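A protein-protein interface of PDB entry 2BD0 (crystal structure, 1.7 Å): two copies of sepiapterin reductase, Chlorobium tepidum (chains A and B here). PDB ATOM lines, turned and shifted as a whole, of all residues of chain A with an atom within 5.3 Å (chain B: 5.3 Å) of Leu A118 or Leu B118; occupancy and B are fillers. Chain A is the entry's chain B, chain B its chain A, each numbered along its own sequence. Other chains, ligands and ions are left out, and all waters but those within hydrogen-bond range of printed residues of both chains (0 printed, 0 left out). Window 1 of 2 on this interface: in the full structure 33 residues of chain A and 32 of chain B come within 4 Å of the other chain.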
ATOM      1  N   PHE A 110      -7.087 -21.717  18.427  1.00  0.00           N
ATOM      2  CA  PHE A 110      -8.426 -22.144  18.815  1.00  0.00           C
ATOM      3  C   PHE A 110      -8.534 -22.448  20.307  1.00  0.00           C
ATOM      4  O   PHE A 110      -9.370 -21.871  21.005  1.00  0.00           O
ATOM      5  CB  PHE A 110      -8.842 -23.372  17.999  1.00  0.00           C
ATOM      6  CG  PHE A 110     -10.257 -23.810  18.250  1.00  0.00           C
ATOM      7  CD1 PHE A 110     -10.573 -24.594  19.356  1.00  0.00           C
ATOM      8  CD2 PHE A 110     -11.283 -23.395  17.408  1.00  0.00           C
ATOM      9  CE1 PHE A 110     -11.897 -24.956  19.621  1.00  0.00           C
ATOM     10  CE2 PHE A 110     -12.607 -23.750  17.662  1.00  0.00           C
ATOM     11  CZ  PHE A 110     -12.915 -24.532  18.772  1.00  0.00           C
ATOM     12  N   THR A 113      -8.032 -19.376  22.616  1.00  0.00           N
ATOM     13  CA  THR A 113      -9.200 -18.503  22.617  1.00  0.00           C
ATOM     14  C   THR A 113     -10.374 -19.104  23.389  1.00  0.00           C
ATOM     15  O   THR A 113     -10.958 -18.445  24.251  1.00  0.00           O
ATOM     16  CB  THR A 113      -9.676 -18.193  21.179  1.00  0.00           C
ATOM     17  OG1 THR A 113      -8.603 -17.612  20.430  1.00  0.00           O
ATOM     18  CG2 THR A 113     -10.849 -17.208  21.209  1.00  0.00           C
ATOM     19  N   MET A 114     -10.712 -20.355  23.089  1.00  0.00           N
ATOM     20  CA  MET A 114     -11.843 -21.006  23.743  1.00  0.00           C
ATOM     21  C   MET A 114     -11.662 -21.301  25.226  1.00  0.00           C
ATOM     22  O   MET A 114     -12.607 -21.163  26.000  1.00  0.00           O
ATOM     23  CB  MET A 114     -12.210 -22.294  23.004  1.00  0.00           C
ATOM     24  CG  MET A 114     -12.610 -22.058  21.552  1.00  0.00           C
ATOM     25  SD  MET A 114     -13.891 -20.781  21.387  1.00  0.00           S
ATOM     26  CE  MET A 114     -13.940 -20.579  19.592  1.00  0.00           C
ATOM     27  N   ASN A 115     -10.460 -21.709  25.625  1.00  0.00           N
ATOM     28  CA  ASN A 115     -10.204 -22.012  27.028  1.00  0.00           C
ATOM     29  C   ASN A 115     -10.464 -20.818  27.944  1.00  0.00           C
ATOM     30  O   ASN A 115     -10.868 -20.990  29.092  1.00  0.00           O
ATOM     31  CB  ASN A 115      -8.764 -22.504  27.209  1.00  0.00           C
ATOM     32  CG  ASN A 115      -8.602 -23.977  26.863  1.00  0.00           C
ATOM     33  OD1 ASN A 115      -7.485 -24.452  26.632  1.00  0.00           O
ATOM     34  ND2 ASN A 115      -9.712 -24.712  26.845  1.00  0.00           N
ATOM     35  N   THR A 116     -10.225 -19.611  27.438  1.00  0.00           N
ATOM     36  CA  THR A 116     -10.459 -18.407  28.234  1.00  0.00           C
ATOM     37  C   THR A 116     -11.838 -17.791  28.010  1.00  0.00           C
ATOM     38  O   THR A 116     -12.633 -17.667  28.944  1.00  0.00           O
ATOM     39  CB  THR A 116      -9.406 -17.314  27.939  1.00  0.00           C
ATOM     40  OG1 THR A 116      -8.136 -17.722  28.463  1.00  0.00           O
ATOM     41  CG2 THR A 116      -9.813 -15.990  28.588  1.00  0.00           C
ATOM     42  N   ASN A 117     -12.119 -17.409  26.769  1.00  0.00           N
ATOM     43  CA  ASN A 117     -13.388 -16.767  26.441  1.00  0.00           C
ATOM     44  C   ASN A 117     -14.628 -17.611  26.723  1.00  0.00           C
ATOM     45  O   ASN A 117     -15.651 -17.084  27.168  1.00  0.00           O
ATOM     46  CB  ASN A 117     -13.394 -16.324  24.968  1.00  0.00           C
ATOM     47  CG  ASN A 117     -12.324 -15.283  24.657  1.00  0.00           C
ATOM     48  OD1 ASN A 117     -12.256 -14.760  23.539  1.00  0.00           O
ATOM     49  ND2 ASN A 117     -11.482 -14.983  25.636  1.00  0.00           N
ATOM     50  N   LEU A 118     -14.553 -18.916  26.474  1.00  0.00           N
ATOM     51  CA  LEU A 118     -15.715 -19.765  26.702  1.00  0.00           C
ATOM     52  C   LEU A 118     -15.671 -20.657  27.939  1.00  0.00           C
ATOM     53  O   LEU A 118     -16.545 -20.570  28.799  1.00  0.00           O
ATOM     54  CB  LEU A 118     -15.986 -20.642  25.476  1.00  0.00           C
ATOM     55  CG  LEU A 118     -16.544 -19.963  24.226  1.00  0.00           C
ATOM     56  CD1 LEU A 118     -16.908 -21.034  23.209  1.00  0.00           C
ATOM     57  CD2 LEU A 118     -17.786 -19.139  24.581  1.00  0.00           C
ATOM     58  N   LYS A 119     -14.653 -21.508  28.028  1.00  0.00           N
ATOM     59  CA  LYS A 119     -14.549 -22.437  29.150  1.00  0.00           C
ATOM     60  C   LYS A 119     -14.369 -21.766  30.509  1.00  0.00           C
ATOM     61  O   LYS A 119     -15.176 -21.972  31.415  1.00  0.00           O
ATOM     62  CB  LYS A 119     -13.408 -23.432  28.902  1.00  0.00           C
ATOM     63  CG  LYS A 119     -13.468 -24.653  29.802  1.00  0.00           C
ATOM     64  CD  LYS A 119     -12.452 -25.711  29.381  1.00  0.00           C
ATOM     65  CE  LYS A 119     -12.621 -26.978  30.211  1.00  0.00           C
ATOM     66  NZ  LYS A 119     -11.694 -28.065  29.787  1.00  0.00           N
ATOM     67  N   GLY A 120     -13.316 -20.971  30.649  1.00  0.00           N
ATOM     68  CA  GLY A 120     -13.075 -20.298  31.913  1.00  0.00           C
ATOM     69  C   GLY A 120     -14.252 -19.422  32.299  1.00  0.00           C
ATOM     70  O   GLY A 120     -14.726 -19.447  33.435  1.00  0.00           O
ATOM     71  N   THR A 121     -14.741 -18.649  31.337  1.00  0.00           N
ATOM     72  CA  THR A 121     -15.862 -17.759  31.588  1.00  0.00           C
ATOM     73  C   THR A 121     -17.097 -18.534  32.033  1.00  0.00           C
ATOM     74  O   THR A 121     -17.792 -18.126  32.959  1.00  0.00           O
ATOM     75  CB  THR A 121     -16.181 -16.925  30.328  1.00  0.00           C
ATOM     76  OG1 THR A 121     -15.036 -16.132  29.990  1.00  0.00           O
ATOM     77  CG2 THR A 121     -17.371 -16.005  30.576  1.00  0.00           C
ATOM     78  N   PHE A 122     -17.361 -19.664  31.390  1.00  0.00           N
ATOM     79  CA  PHE A 122     -18.529 -20.456  31.757  1.00  0.00           C
ATOM     80  C   PHE A 122     -18.451 -21.024  33.169  1.00  0.00           C
ATOM     81  O   PHE A 122     -19.379 -20.875  33.961  1.00  0.00           O
ATOM     82  CB  PHE A 122     -18.726 -21.624  30.795  1.00  0.00           C
ATOM     83  CG  PHE A 122     -19.825 -22.556  31.217  1.00  0.00           C
ATOM     84  CD1 PHE A 122     -21.157 -22.200  31.047  1.00  0.00           C
ATOM     85  CD2 PHE A 122     -19.528 -23.763  31.844  1.00  0.00           C
ATOM     86  CE1 PHE A 122     -22.184 -23.027  31.498  1.00  0.00           C
ATOM     87  CE2 PHE A 122     -20.548 -24.600  32.302  1.00  0.00           C
ATOM     88  CZ  PHE A 122     -21.878 -24.231  32.128  1.00  0.00           C
ATOM     89  N   PHE A 123     -17.346 -21.685  33.488  1.00  0.00           N
ATOM     90  CA  PHE A 123     -17.233 -22.296  34.801  1.00  0.00           C
ATOM     91  C   PHE A 123     -17.142 -21.326  35.963  1.00  0.00           C
ATOM     92  O   PHE A 123     -17.631 -21.625  37.053  1.00  0.00           O
ATOM     93  CB  PHE A 123     -16.096 -23.317  34.789  1.00  0.00           C
ATOM     94  CG  PHE A 123     -16.462 -24.571  34.049  1.00  0.00           C
ATOM     95  CD1 PHE A 123     -17.409 -25.443  34.581  1.00  0.00           C
ATOM     96  CD2 PHE A 123     -15.971 -24.815  32.770  1.00  0.00           C
ATOM     97  CE1 PHE A 123     -17.872 -26.532  33.851  1.00  0.00           C
ATOM     98  CE2 PHE A 123     -16.428 -25.905  32.029  1.00  0.00           C
ATOM     99  CZ  PHE A 123     -17.383 -26.762  32.572  1.00  0.00           C
ATOM    100  N   MET A 160     -16.410 -16.853  16.874  1.00  0.00           N
ATOM    101  CA  MET A 160     -16.992 -18.086  17.392  1.00  0.00           C
ATOM    102  C   MET A 160     -17.069 -17.981  18.914  1.00  0.00           C
ATOM    103  O   MET A 160     -18.086 -18.325  19.510  1.00  0.00           O
ATOM    104  CB  MET A 160     -16.145 -19.305  17.012  1.00  0.00           C
ATOM    105  CG  MET A 160     -16.382 -19.804  15.597  1.00  0.00           C
ATOM    106  SD  MET A 160     -15.443 -21.300  15.215  1.00  0.00           S
ATOM    107  CE  MET A 160     -16.452 -22.512  15.872  1.00  0.00           C
ATOM    108  N   SER A 161     -16.005 -17.469  19.531  1.00  0.00           N
ATOM    109  CA  SER A 161     -15.963 -17.352  20.987  1.00  0.00           C
ATOM    110  C   SER A 161     -16.873 -16.264  21.543  1.00  0.00           C
ATOM    111  O   SER A 161     -17.456 -16.437  22.611  1.00  0.00           O
ATOM    112  CB  SER A 161     -14.522 -17.116  21.477  1.00  0.00           C
ATOM    113  OG  SER A 161     -14.105 -15.767  21.315  1.00  0.00           O
ATOM    114  N   GLY A 164     -20.407 -17.203  21.021  1.00  0.00           N
ATOM    115  CA  GLY A 164     -20.560 -18.210  22.057  1.00  0.00           C
ATOM    116  C   GLY A 164     -20.851 -17.590  23.413  1.00  0.00           C
ATOM    117  O   GLY A 164     -21.724 -18.068  24.142  1.00  0.00           O
ATOM    118  N   GLN A 165     -20.118 -16.539  23.771  1.00  0.00           N
ATOM    119  CA  GLN A 165     -20.360 -15.879  25.053  1.00  0.00           C
ATOM    120  C   GLN A 165     -21.794 -15.364  25.105  1.00  0.00           C
ATOM    121  O   GLN A 165     -22.453 -15.459  26.138  1.00  0.00           O
ATOM    122  CB  GLN A 165     -19.398 -14.704  25.273  1.00  0.00           C
ATOM    123  CG  GLN A 165     -17.939 -15.092  25.462  1.00  0.00           C
ATOM    124  CD  GLN A 165     -17.108 -13.957  26.045  1.00  0.00           C
ATOM    125  OE1 GLN A 165     -17.338 -12.783  25.746  1.00  0.00           O
ATOM    126  NE2 GLN A 165     -16.125 -14.307  26.870  1.00  0.00           N
ATOM    127  N   PHE B 110     -18.760 -29.902  28.576  1.00  0.00           N
ATOM    128  CA  PHE B 110     -18.242 -28.771  27.821  1.00  0.00           C
ATOM    129  C   PHE B 110     -17.282 -29.204  26.717  1.00  0.00           C
ATOM    130  O   PHE B 110     -17.495 -28.893  25.541  1.00  0.00           O
ATOM    131  CB  PHE B 110     -17.553 -27.781  28.773  1.00  0.00           C
ATOM    132  CG  PHE B 110     -17.033 -26.552  28.092  1.00  0.00           C
ATOM    133  CD1 PHE B 110     -15.809 -26.568  27.428  1.00  0.00           C
ATOM    134  CD2 PHE B 110     -17.794 -25.385  28.068  1.00  0.00           C
ATOM    135  CE1 PHE B 110     -15.348 -25.439  26.747  1.00  0.00           C
ATOM    136  CE2 PHE B 110     -17.343 -24.250  27.389  1.00  0.00           C
ATOM    137  CZ  PHE B 110     -16.119 -24.279  26.729  1.00  0.00           C
ATOM    138  N   THR B 113     -18.905 -31.353  23.891  1.00  0.00           N
ATOM    139  CA  THR B 113     -19.719 -30.534  23.003  1.00  0.00           C
ATOM    140  C   THR B 113     -18.872 -29.659  22.082  1.00  0.00           C
ATOM    141  O   THR B 113     -19.075 -29.644  20.866  1.00  0.00           O
ATOM    142  CB  THR B 113     -20.675 -29.618  23.809  1.00  0.00           C
ATOM    143  OG1 THR B 113     -21.544 -30.425  24.615  1.00  0.00           O
ATOM    144  CG2 THR B 113     -21.525 -28.764  22.862  1.00  0.00           C
ATOM    145  N   MET B 114     -17.907 -28.944  22.653  1.00  0.00           N
ATOM    146  CA  MET B 114     -17.082 -28.045  21.851  1.00  0.00           C
ATOM    147  C   MET B 114     -16.127 -28.733  20.882  1.00  0.00           C
ATOM    148  O   MET B 114     -15.895 -28.233  19.781  1.00  0.00           O
ATOM    149  CB  MET B 114     -16.298 -27.090  22.757  1.00  0.00           C
ATOM    150  CG  MET B 114     -17.169 -26.219  23.651  1.00  0.00           C
ATOM    151  SD  MET B 114     -18.542 -25.419  22.778  1.00  0.00           S
ATOM    152  CE  MET B 114     -19.424 -24.681  24.155  1.00  0.00           C
ATOM    153  N   ASN B 115     -15.573 -29.874  21.284  1.00  0.00           N
ATOM    154  CA  ASN B 115     -14.642 -30.599  20.428  1.00  0.00           C
ATOM    155  C   ASN B 115     -15.275 -30.982  19.095  1.00  0.00           C
ATOM    156  O   ASN B 115     -14.594 -31.032  18.077  1.00  0.00           O
ATOM    157  CB  ASN B 115     -14.125 -31.858  21.139  1.00  0.00           C
ATOM    158  CG  ASN B 115     -13.000 -31.556  22.115  1.00  0.00           C
ATOM    159  OD1 ASN B 115     -12.702 -32.357  23.010  1.00  0.00           O
ATOM    160  ND2 ASN B 115     -12.358 -30.406  21.941  1.00  0.00           N
ATOM    161  N   THR B 116     -16.575 -31.258  19.098  1.00  0.00           N
ATOM    162  CA  THR B 116     -17.256 -31.616  17.855  1.00  0.00           C
ATOM    163  C   THR B 116     -17.938 -30.416  17.195  1.00  0.00           C
ATOM    164  O   THR B 116     -17.650 -30.074  16.049  1.00  0.00           O
ATOM    165  CB  THR B 116     -18.334 -32.705  18.083  1.00  0.00           C
ATOM    166  OG1 THR B 116     -17.703 -33.953  18.407  1.00  0.00           O
ATOM    167  CG2 THR B 116     -19.181 -32.888  16.824  1.00  0.00           C
ATOM    168  N   ASN B 117     -18.833 -29.771  17.936  1.00  0.00           N
ATOM    169  CA  ASN B 117     -19.594 -28.645  17.404  1.00  0.00           C
ATOM    170  C   ASN B 117     -18.772 -27.443  16.955  1.00  0.00           C
ATOM    171  O   ASN B 117     -19.112 -26.798  15.965  1.00  0.00           O
ATOM    172  CB  ASN B 117     -20.651 -28.196  18.426  1.00  0.00           C
ATOM    173  CG  ASN B 117     -21.708 -29.259  18.687  1.00  0.00           C
ATOM    174  OD1 ASN B 117     -22.686 -29.022  19.405  1.00  0.00           O
ATOM    175  ND2 ASN B 117     -21.518 -30.435  18.110  1.00  0.00           N
ATOM    176  N   LEU B 118     -17.703 -27.125  17.675  1.00  0.00           N
ATOM    177  CA  LEU B 118     -16.890 -25.975  17.299  1.00  0.00           C
ATOM    178  C   LEU B 118     -15.535 -26.321  16.714  1.00  0.00           C
ATOM    179  O   LEU B 118     -15.198 -25.872  15.624  1.00  0.00           O
ATOM    180  CB  LEU B 118     -16.680 -25.041  18.494  1.00  0.00           C
ATOM    181  CG  LEU B 118     -17.908 -24.347  19.088  1.00  0.00           C
ATOM    182  CD1 LEU B 118     -17.440 -23.373  20.166  1.00  0.00           C
ATOM    183  CD2 LEU B 118     -18.686 -23.604  18.006  1.00  0.00           C
ATOM    184  N   LYS B 119     -14.757 -27.127  17.431  1.00  0.00           N
ATOM    185  CA  LYS B 119     -13.414 -27.465  16.968  1.00  0.00           C
ATOM    186  C   LYS B 119     -13.365 -28.302  15.688  1.00  0.00           C
ATOM    187  O   LYS B 119     -12.759 -27.888  14.702  1.00  0.00           O
ATOM    188  CB  LYS B 119     -12.637 -28.168  18.083  1.00  0.00           C
ATOM    189  CG  LYS B 119     -11.140 -28.237  17.815  1.00  0.00           C
ATOM    190  CD  LYS B 119     -10.366 -28.627  19.070  1.00  0.00           C
ATOM    191  CE  LYS B 119      -8.869 -28.644  18.798  1.00  0.00           C
ATOM    192  NZ  LYS B 119      -8.101 -28.913  20.055  1.00  0.00           N
ATOM    193  N   GLY B 120     -13.998 -29.469  15.702  1.00  0.00           N
ATOM    194  CA  GLY B 120     -13.993 -30.307  14.514  1.00  0.00           C
ATOM    195  C   GLY B 120     -14.640 -29.583  13.348  1.00  0.00           C
ATOM    196  O   GLY B 120     -14.137 -29.595  12.227  1.00  0.00           O
ATOM    197  N   THR B 121     -15.771 -28.945  13.613  1.00  0.00           N
ATOM    198  CA  THR B 121     -16.464 -28.222  12.567  1.00  0.00           C
ATOM    199  C   THR B 121     -15.569 -27.136  11.962  1.00  0.00           C
ATOM    200  O   THR B 121     -15.489 -27.005  10.744  1.00  0.00           O
ATOM    201  CB  THR B 121     -17.766 -27.608  13.103  1.00  0.00           C
ATOM    202  OG1 THR B 121     -18.635 -28.664  13.540  1.00  0.00           O
ATOM    203  CG2 THR B 121     -18.464 -26.798  12.013  1.00  0.00           C
ATOM    204  N   PHE B 122     -14.884 -26.368  12.805  1.00  0.00           N
ATOM    205  CA  PHE B 122     -14.009 -25.311  12.297  1.00  0.00           C
ATOM    206  C   PHE B 122     -12.873 -25.824  11.414  1.00  0.00           C
ATOM    207  O   PHE B 122     -12.691 -25.361  10.291  1.00  0.00           O
ATOM    208  CB  PHE B 122     -13.381 -24.509  13.441  1.00  0.00           C
ATOM    209  CG  PHE B 122     -12.433 -23.433  12.968  1.00  0.00           C
ATOM    210  CD1 PHE B 122     -12.921 -22.261  12.400  1.00  0.00           C
ATOM    211  CD2 PHE B 122     -11.055 -23.616  13.041  1.00  0.00           C
ATOM    212  CE1 PHE B 122     -12.052 -21.285  11.905  1.00  0.00           C
ATOM    213  CE2 PHE B 122     -10.179 -22.652  12.552  1.00  0.00           C
ATOM    214  CZ  PHE B 122     -10.675 -21.485  11.983  1.00  0.00           C
ATOM    215  N   PHE B 123     -12.099 -26.776  11.918  1.00  0.00           N
ATOM    216  CA  PHE B 123     -10.979 -27.264  11.130  1.00  0.00           C
ATOM    217  C   PHE B 123     -11.347 -28.029   9.870  1.00  0.00           C
ATOM    218  O   PHE B 123     -10.597 -27.999   8.897  1.00  0.00           O
ATOM    219  CB  PHE B 123     -10.021 -28.038  12.035  1.00  0.00           C
ATOM    220  CG  PHE B 123      -9.282 -27.144  12.984  1.00  0.00           C
ATOM    221  CD1 PHE B 123      -8.312 -26.263  12.509  1.00  0.00           C
ATOM    222  CD2 PHE B 123      -9.627 -27.094  14.331  1.00  0.00           C
ATOM    223  CE1 PHE B 123      -7.705 -25.340  13.356  1.00  0.00           C
ATOM    224  CE2 PHE B 123      -9.022 -26.170  15.186  1.00  0.00           C
ATOM    225  CZ  PHE B 123      -8.063 -25.295  14.697  1.00  0.00           C
ATOM    226  N   MET B 160     -24.005 -22.175  23.788  1.00  0.00           N
ATOM    227  CA  MET B 160     -22.700 -21.568  23.565  1.00  0.00           C
ATOM    228  C   MET B 160     -22.121 -22.146  22.271  1.00  0.00           C
ATOM    229  O   MET B 160     -21.558 -21.420  21.453  1.00  0.00           O
ATOM    230  CB  MET B 160     -21.733 -21.864  24.718  1.00  0.00           C
ATOM    231  CG  MET B 160     -21.965 -21.028  25.967  1.00  0.00           C
ATOM    232  SD  MET B 160     -20.615 -21.213  27.169  1.00  0.00           S
ATOM    233  CE  MET B 160     -20.969 -22.859  27.801  1.00  0.00           C
ATOM    234  N   SER B 161     -22.290 -23.452  22.076  1.00  0.00           N
ATOM    235  CA  SER B 161     -21.741 -24.102  20.891  1.00  0.00           C
ATOM    236  C   SER B 161     -22.478 -23.753  19.605  1.00  0.00           C
ATOM    237  O   SER B 161     -21.857 -23.643  18.550  1.00  0.00           O
ATOM    238  CB  SER B 161     -21.709 -25.629  21.074  1.00  0.00           C
ATOM    239  OG  SER B 161     -22.967 -26.223  20.798  1.00  0.00           O
ATOM    240  N   GLY B 164     -21.966 -20.204  18.799  1.00  0.00           N
ATOM    241  CA  GLY B 164     -20.600 -20.226  18.301  1.00  0.00           C
ATOM    242  C   GLY B 164     -20.532 -20.644  16.844  1.00  0.00           C
ATOM    243  O   GLY B 164     -19.797 -20.041  16.055  1.00  0.00           O
ATOM    244  N   GLN B 165     -21.281 -21.683  16.477  1.00  0.00           N
ATOM    245  CA  GLN B 165     -21.282 -22.131  15.085  1.00  0.00           C
ATOM    246  C   GLN B 165     -21.769 -21.000  14.189  1.00  0.00           C
ATOM    247  O   GLN B 165     -21.252 -20.807  13.096  1.00  0.00           O
ATOM    248  CB  GLN B 165     -22.196 -23.345  14.884  1.00  0.00           C
ATOM    249  CG  GLN B 165     -21.703 -24.637  15.524  1.00  0.00           C
ATOM    250  CD  GLN B 165     -22.459 -25.851  15.010  1.00  0.00           C
ATOM    251  OE1 GLN B 165     -23.680 -25.806  14.826  1.00  0.00           O
ATOM    252  NE2 GLN B 165     -21.739 -26.947  14.785  1.00  0.00           N
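The backbone carbonyl oxygen (O) of Met B114 lies within hydrogen-bond range of the backbone NH (N) of Lys B119 (2.8 Å).
The backbone carbonyl oxygen (O) of Met A114 is in hydrogen-bond range of the backbone NH (N) of Lys A119 (2.9 Å).
Among the printed residues, pairs that only touch across the chains: Met A160 with Leu B118 (3.3 Å), Phe A122 with Met B160 (3.3 Å), Met A160 with Gly B164 (3.4 Å), Lys A119 with Phe B110 (3.4 Å), Gly A164 with Met B160 (3.4 Å), Phe A110 with Lys B119 (3.5 Å), Phe A110 with Leu B118 (3.8 Å), Leu A118 with Phe B110 (3.8 Å), Leu A118 with Leu B118 (3.9 Å), Phe A110 with Phe B123 (3.9 Å), Met A160 with Phe B122 (3.9 Å) and Phe A123 with Phe B110 (3.9 Å).
Of chain B, only Phe B110 and Leu B118 come within 4 Å of Leu A118.
Leu B118 touches three residues of chain A.
Printed residues of chain A within 4 Å of Phe B122: Met A160 (3.9 Å).
Of the printed residues of chain A, Gly B164 touches Met A160.
Of the printed residues of chain A, Phe B110 touches Leu A118, Lys A119 and Phe A123.
Printed residues of chain B within 4 Å of Phe A110: Leu B118, Lys B119 and Phe B123.
Ser B161 touches none of the printed residues of chain A.
Thr A121 touches none of the printed residues of chain B.
The nearest residue of chain B that does not touch Leu A118 is Met B160 (4.4 Å).
The nearest residue of chain A that does not touch Leu B118 is Met A114 (4.5 Å).
The nearest printed residue of chain B that does not touch Gly A164 is Gly B164 (4.05 Å).
Phe A110 touches Phe B123, and with the chains exchanged Phe A123 touches Phe B110.
Leu B118 touches its own counterpart, Leu A118.
Phe A122 touches Met B160, and with the chains exchanged Met A160 touches Phe B122.
Met A160 touches Leu B118, but with the chains exchanged Leu A118 does not touch Met B160 (4.4 Å).
Of the 12 pairs that touch across the chains among the printed residues, 11 have their exchanged pair printed and touching as well.
Printed residues of chain A that touch a printed residue of chain B: Phe A110, Leu A118, Lys A119, Phe A122, Phe A123, Met A160 and Gly A164.
Printed residues of chain B that touch a printed residue of chain A: Phe B110, Leu B118, Lys B119, Phe B122, Phe B123, Met B160 and Gly B164.
Hydrophobic or aromatic side chains of chain B within 4 Å of the printed part of chain A: Phe B110, Leu B118, Phe B122, Phe B123 and Met B160.
Along chain B the printed residues that touch a printed residue of chain A span positions 110 to 164.
Among the printed residues, 12 pairs touch across the chains.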
